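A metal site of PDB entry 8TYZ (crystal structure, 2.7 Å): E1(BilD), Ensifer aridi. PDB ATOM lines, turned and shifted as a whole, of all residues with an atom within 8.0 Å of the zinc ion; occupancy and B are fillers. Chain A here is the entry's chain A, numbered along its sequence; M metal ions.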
ATOM      1  N   GLN A 310     -12.063  19.359 -14.886  1.00  0.00           N
ATOM      2  CA  GLN A 310     -10.908  19.359 -15.767  1.00  0.00           C
ATOM      3  C   GLN A 310      -9.588  19.377 -14.984  1.00  0.00           C
ATOM      4  O   GLN A 310      -8.599  18.765 -15.407  1.00  0.00           O
ATOM      5  CB  GLN A 310     -10.964  20.570 -16.708  1.00  0.00           C
ATOM      6  CG  GLN A 310      -9.836  20.603 -17.707  1.00  0.00           C
ATOM      7  CD  GLN A 310      -9.928  19.466 -18.692  1.00  0.00           C
ATOM      8  OE1 GLN A 310      -9.476  18.344 -18.438  1.00  0.00           O
ATOM      9  NE2 GLN A 310     -10.541  19.737 -19.823  1.00  0.00           N
ATOM     10  N   HIS A 332     -13.659  16.952 -24.930  1.00  0.00           N
ATOM     11  CA  HIS A 332     -12.380  17.454 -24.432  1.00  0.00           C
ATOM     12  C   HIS A 332     -11.428  16.330 -24.045  1.00  0.00           C
ATOM     13  O   HIS A 332     -11.619  15.655 -23.036  1.00  0.00           O
ATOM     14  CB  HIS A 332     -12.604  18.375 -23.235  1.00  0.00           C
ATOM     15  CG  HIS A 332     -13.535  19.507 -23.509  1.00  0.00           C
ATOM     16  ND1 HIS A 332     -13.193  20.584 -24.302  1.00  0.00           N
ATOM     17  CD2 HIS A 332     -14.814  19.718 -23.109  1.00  0.00           C
ATOM     18  CE1 HIS A 332     -14.216  21.407 -24.371  1.00  0.00           C
ATOM     19  NE2 HIS A 332     -15.210  20.913 -23.655  1.00  0.00           N
ATOM     20  N   GLY A 333     -10.406  16.128 -24.840  1.00  0.00           N
ATOM     21  CA  GLY A 333      -9.167  15.580 -24.346  1.00  0.00           C
ATOM     22  C   GLY A 333      -8.252  16.750 -24.015  1.00  0.00           C
ATOM     23  O   GLY A 333      -8.446  17.868 -24.514  1.00  0.00           O
ATOM     24  N   PHE A 334      -7.269  16.499 -23.170  1.00  0.00           N
ATOM     25  CA  PHE A 334      -6.471  17.617 -22.677  1.00  0.00           C
ATOM     26  C   PHE A 334      -5.222  17.846 -23.531  1.00  0.00           C
ATOM     27  O   PHE A 334      -4.860  19.000 -23.797  1.00  0.00           O
ATOM     28  CB  PHE A 334      -6.083  17.340 -21.230  1.00  0.00           C
ATOM     29  CG  PHE A 334      -5.477  18.501 -20.523  1.00  0.00           C
ATOM     30  CD1 PHE A 334      -6.270  19.546 -20.119  1.00  0.00           C
ATOM     31  CD2 PHE A 334      -4.141  18.497 -20.206  1.00  0.00           C
ATOM     32  CE1 PHE A 334      -5.714  20.593 -19.431  1.00  0.00           C
ATOM     33  CE2 PHE A 334      -3.576  19.546 -19.530  1.00  0.00           C
ATOM     34  CZ  PHE A 334      -4.357  20.577 -19.137  1.00  0.00           C
ATOM     35  N   GLN A 338      -6.698  20.552 -29.213  1.00  0.00           N
ATOM     36  CA  GLN A 338      -7.992  21.206 -29.198  1.00  0.00           C
ATOM     37  C   GLN A 338      -8.248  21.849 -27.830  1.00  0.00           C
ATOM     38  O   GLN A 338      -7.456  21.715 -26.893  1.00  0.00           O
ATOM     39  CB  GLN A 338      -9.095  20.214 -29.542  1.00  0.00           C
ATOM     40  CG  GLN A 338      -8.753  19.306 -30.685  1.00  0.00           C
ATOM     41  CD  GLN A 338      -8.538  20.103 -31.944  1.00  0.00           C
ATOM     42  OE1 GLN A 338      -9.304  21.033 -32.242  1.00  0.00           O
ATOM     43  NE2 GLN A 338      -7.479  19.769 -32.693  1.00  0.00           N
ATOM     44  N   ALA A 339      -9.380  22.540 -27.739  1.00  0.00           N
ATOM     45  CA  ALA A 339      -9.800  23.142 -26.478  1.00  0.00           C
ATOM     46  C   ALA A 339     -10.062  22.073 -25.413  1.00  0.00           C
ATOM     47  O   ALA A 339     -10.429  20.939 -25.695  1.00  0.00           O
ATOM     48  CB  ALA A 339     -11.059  23.982 -26.671  1.00  0.00           C
ATOM     49  N   CYS A 340      -9.811  22.462 -24.179  1.00  0.00           N
ATOM     50  CA  CYS A 340     -10.128  21.664 -23.003  1.00  0.00           C
ATOM     51  C   CYS A 340     -11.398  22.220 -22.388  1.00  0.00           C
ATOM     52  O   CYS A 340     -11.924  23.253 -22.826  1.00  0.00           O
ATOM     53  CB  CYS A 340      -8.972  21.695 -22.018  1.00  0.00           C
ATOM     54  SG  CYS A 340      -8.842  23.216 -21.099  1.00  0.00           S
ATOM     55  N   LEU A 341     -11.901  21.555 -21.354  1.00  0.00           N
ATOM     56  CA  LEU A 341     -13.132  22.036 -20.723  1.00  0.00           C
ATOM     57  C   LEU A 341     -12.936  23.416 -20.144  1.00  0.00           C
ATOM     58  O   LEU A 341     -13.883  24.213 -20.128  1.00  0.00           O
ATOM     59  CB  LEU A 341     -13.615  21.077 -19.638  1.00  0.00           C
ATOM     60  CG  LEU A 341     -14.965  21.458 -19.015  1.00  0.00           C
ATOM     61  CD1 LEU A 341     -15.938  21.712 -20.120  1.00  0.00           C
ATOM     62  CD2 LEU A 341     -15.477  20.340 -18.093  1.00  0.00           C
ATOM     63  N   CYS A 342     -11.726  23.726 -19.682  1.00  0.00           N
ATOM     64  CA  CYS A 342     -11.494  25.028 -19.064  1.00  0.00           C
ATOM     65  C   CYS A 342     -11.540  26.159 -20.099  1.00  0.00           C
ATOM     66  O   CYS A 342     -11.934  27.285 -19.757  1.00  0.00           O
ATOM     67  CB  CYS A 342     -10.170  25.002 -18.306  1.00  0.00           C
ATOM     68  SG  CYS A 342      -9.869  26.387 -17.194  1.00  0.00           S
ATOM     69  N   CYS A 343     -11.165  25.879 -21.351  1.00  0.00           N
ATOM     70  CA  CYS A 343     -11.212  26.883 -22.416  1.00  0.00           C
ATOM     71  C   CYS A 343     -12.618  27.417 -22.586  1.00  0.00           C
ATOM     72  O   CYS A 343     -12.824  28.623 -22.787  1.00  0.00           O
ATOM     73  CB  CYS A 343     -10.750  26.283 -23.753  1.00  0.00           C
ATOM     74  SG  CYS A 343      -9.034  25.791 -23.839  1.00  0.00           S
ATOM     75  N   MET A 344     -13.602  26.537 -22.462  1.00  0.00           N
ATOM     76  CA  MET A 344     -14.996  26.882 -22.674  1.00  0.00           C
ATOM     77  C   MET A 344     -15.480  27.939 -21.697  1.00  0.00           C
ATOM     78  O   MET A 344     -16.428  28.671 -22.012  1.00  0.00           O
ATOM     79  CB  MET A 344     -15.820  25.603 -22.557  1.00  0.00           C
ATOM     80  CG  MET A 344     -15.242  24.489 -23.395  1.00  0.00           C
ATOM     81  SD  MET A 344     -15.298  24.835 -25.166  1.00  0.00           S
ATOM     82  CE  MET A 344     -17.027  25.273 -25.271  1.00  0.00           C
ATOM     83  N   TYR A 345     -14.867  28.037 -20.529  1.00  0.00           N
ATOM     84  CA  TYR A 345     -15.380  28.927 -19.511  1.00  0.00           C
ATOM     85  C   TYR A 345     -14.364  29.981 -19.105  1.00  0.00           C
ATOM     86  O   TYR A 345     -14.642  30.758 -18.189  1.00  0.00           O
ATOM     87  CB  TYR A 345     -15.876  28.115 -18.300  1.00  0.00           C
ATOM     88  CG  TYR A 345     -16.994  27.183 -18.699  1.00  0.00           C
ATOM     89  CD1 TYR A 345     -18.306  27.659 -18.889  1.00  0.00           C
ATOM     90  CD2 TYR A 345     -16.748  25.832 -18.935  1.00  0.00           C
ATOM     91  CE1 TYR A 345     -19.338  26.820 -19.296  1.00  0.00           C
ATOM     92  CE2 TYR A 345     -17.771  24.989 -19.346  1.00  0.00           C
ATOM     93  CZ  TYR A 345     -19.067  25.492 -19.526  1.00  0.00           C
ATOM     94  OH  TYR A 345     -20.068  24.641 -19.930  1.00  0.00           O
ATOM     95  N   MET A 346     -13.238  30.081 -19.810  1.00  0.00           N
ATOM     96  CA  MET A 346     -12.232  31.100 -19.512  1.00  0.00           C
ATOM     97  C   MET A 346     -12.871  32.487 -19.442  1.00  0.00           C
ATOM     98  O   MET A 346     -13.822  32.771 -20.178  1.00  0.00           O
ATOM     99  CB  MET A 346     -11.145  31.100 -20.580  1.00  0.00           C
ATOM    100  CG  MET A 346     -10.107  30.039 -20.359  1.00  0.00           C
ATOM    101  SD  MET A 346      -9.159  30.222 -18.830  1.00  0.00           S
ATOM    102  CE  MET A 346      -7.968  31.481 -19.255  1.00  0.00           C
ATOM    103  N   ALA A 484     -11.776  27.081 -30.468  1.00  0.00           N
ATOM    104  CA  ALA A 484     -10.336  26.879 -30.565  1.00  0.00           C
ATOM    105  C   ALA A 484      -9.718  26.898 -29.188  1.00  0.00           C
ATOM    106  O   ALA A 484     -10.270  27.455 -28.232  1.00  0.00           O
ATOM    107  CB  ALA A 484      -9.709  27.957 -31.440  1.00  0.00           C
ATOM    108  N   LYS A 485      -8.539  26.279 -29.085  1.00  0.00           N
ATOM    109  CA  LYS A 485      -7.814  26.268 -27.822  1.00  0.00           C
ATOM    110  C   LYS A 485      -7.586  27.690 -27.338  1.00  0.00           C
ATOM    111  O   LYS A 485      -7.275  28.578 -28.134  1.00  0.00           O
ATOM    112  CB  LYS A 485      -6.482  25.520 -27.994  1.00  0.00           C
ATOM    113  CG  LYS A 485      -5.718  25.239 -26.723  1.00  0.00           C
ATOM    114  CD  LYS A 485      -4.473  24.463 -27.066  1.00  0.00           C
ATOM    115  CE  LYS A 485      -4.018  23.607 -25.902  1.00  0.00           C
ATOM    116  NZ  LYS A 485      -2.754  22.919 -26.275  1.00  0.00           N
ATOM    117  N   ASP A 486      -7.780  27.919 -26.032  1.00  0.00           N
ATOM    118  CA  ASP A 486      -7.535  29.261 -25.524  1.00  0.00           C
ATOM    119  C   ASP A 486      -6.066  29.613 -25.713  1.00  0.00           C
ATOM    120  O   ASP A 486      -5.187  28.745 -25.570  1.00  0.00           O
ATOM    121  CB  ASP A 486      -7.938  29.385 -24.051  1.00  0.00           C
ATOM    122  CG  ASP A 486      -7.727  30.800 -23.508  1.00  0.00           C
ATOM    123  OD1 ASP A 486      -7.178  31.663 -24.226  1.00  0.00           O
ATOM    124  OD2 ASP A 486      -8.097  31.078 -22.364  1.00  0.00           O
ATOM    125  N   SER A 487      -5.814  30.881 -26.044  1.00  0.00           N
ATOM    126  CA  SER A 487      -4.514  31.362 -26.510  1.00  0.00           C
ATOM    127  C   SER A 487      -3.897  32.410 -25.597  1.00  0.00           C
ATOM    128  O   SER A 487      -2.795  32.883 -25.893  1.00  0.00           O
ATOM    129  CB  SER A 487      -4.659  31.954 -27.917  1.00  0.00           C
ATOM    130  OG  SER A 487      -5.552  33.054 -27.889  1.00  0.00           O
ATOM    131  N   ARG A 490      -3.135  31.569 -20.216  1.00  0.00           N
ATOM    132  CA  ARG A 490      -3.592  31.484 -18.844  1.00  0.00           C
ATOM    133  C   ARG A 490      -4.462  30.255 -18.567  1.00  0.00           C
ATOM    134  O   ARG A 490      -4.784  29.999 -17.403  1.00  0.00           O
ATOM    135  CB  ARG A 490      -4.338  32.765 -18.486  1.00  0.00           C
ATOM    136  CG  ARG A 490      -3.503  33.997 -18.736  1.00  0.00           C
ATOM    137  CD  ARG A 490      -4.211  35.290 -18.354  1.00  0.00           C
ATOM    138  NE  ARG A 490      -5.635  35.260 -18.677  1.00  0.00           N
ATOM    139  CZ  ARG A 490      -6.206  35.884 -19.702  1.00  0.00           C
ATOM    140  NH1 ARG A 490      -5.493  36.595 -20.571  1.00  0.00           N
ATOM    141  NH2 ARG A 490      -7.528  35.787 -19.882  1.00  0.00           N
ATOM    142  N   CYS A 491      -4.832  29.492 -19.585  1.00  0.00           N
ATOM    143  CA  CYS A 491      -5.604  28.275 -19.373  1.00  0.00           C
ATOM    144  C   CYS A 491      -4.673  27.143 -18.940  1.00  0.00           C
ATOM    145  O   CYS A 491      -3.485  27.138 -19.246  1.00  0.00           O
ATOM    146  CB  CYS A 491      -6.358  27.893 -20.656  1.00  0.00           C
ATOM    147  SG  CYS A 491      -7.660  26.626 -20.492  1.00  0.00           S
ATOM    148  N   ILE A 492      -5.249  26.158 -18.235  1.00  0.00           N
ATOM    149  CA  ILE A 492      -4.457  25.057 -17.713  1.00  0.00           C
ATOM    150  C   ILE A 492      -4.000  24.109 -18.808  1.00  0.00           C
ATOM    151  O   ILE A 492      -3.086  23.305 -18.557  1.00  0.00           O
ATOM    152  CB  ILE A 492      -5.216  24.302 -16.594  1.00  0.00           C
ATOM    153  CG1 ILE A 492      -6.525  23.688 -17.096  1.00  0.00           C
ATOM    154  CG2 ILE A 492      -5.513  25.191 -15.400  1.00  0.00           C
ATOM    155  CD1 ILE A 492      -7.228  22.861 -16.050  1.00  0.00           C
ATOM    156  N   CYS A 493      -4.553  24.180 -20.029  1.00  0.00           N
ATOM    157  CA  CYS A 493      -4.021  23.321 -21.098  1.00  0.00           C
ATOM    158  C   CYS A 493      -2.786  23.916 -21.759  1.00  0.00           C
ATOM    159  O   CYS A 493      -2.189  23.248 -22.611  1.00  0.00           O
ATOM    160  CB  CYS A 493      -5.074  23.002 -22.167  1.00  0.00           C
ATOM    161  SG  CYS A 493      -5.914  24.405 -22.919  1.00  0.00           S
ATOM    162  N   SER A 494      -2.379  25.107 -21.348  1.00  0.00           N
ATOM    163  CA  SER A 494      -1.107  25.723 -21.714  1.00  0.00           C
ATOM    164  C   SER A 494       0.000  25.346 -20.749  1.00  0.00           C
ATOM    165  O   SER A 494       1.178  25.518 -21.089  1.00  0.00           O
ATOM    166  CB  SER A 494      -1.227  27.258 -21.750  1.00  0.00           C
ATOM    167  OG  SER A 494      -2.303  27.706 -22.560  1.00  0.00           O
ATOM    168  N   ASP A 495      -0.353  24.835 -19.567  1.00  0.00           N
ATOM    169  CA  ASP A 495       0.571  24.712 -18.444  1.00  0.00           C
ATOM    170  C   ASP A 495       1.350  23.402 -18.483  1.00  0.00           C
ATOM    171  O   ASP A 495       0.748  22.322 -18.491  1.00  0.00           O
ATOM    172  CB  ASP A 495      -0.215  24.823 -17.141  1.00  0.00           C
ATOM    173  CG  ASP A 495       0.680  24.948 -15.939  1.00  0.00           C
ATOM    174  OD1 ASP A 495       1.556  24.088 -15.749  1.00  0.00           O
ATOM    175  OD2 ASP A 495       0.498  25.932 -15.186  1.00  0.00           O
HETATM  176 ZN    ZN M   1      -7.848  25.038 -22.023  1.00  0.00          ZN
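N of Cys 342 sits close to SG of Cys 340 (3.3 Å).
The backbone carbonyl oxygen (O) of Cys 340 lies close to a ring nitrogen (ND1) of His 332.
SG of Cys 343 sits close to N of Asp 486, 3.3 Å away.
The side-chain sulfur (SG) of Cys 491 is bound to the zinc ion (2.2 Å).
SG of Cys 493 binds the zinc ion (2.2 Å).
SG of Cys 340 binds the zinc ion (2.3 Å).
The zinc ion is bound by the side-chain sulfur (SG) of Cys 343, at 2.3 Å.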
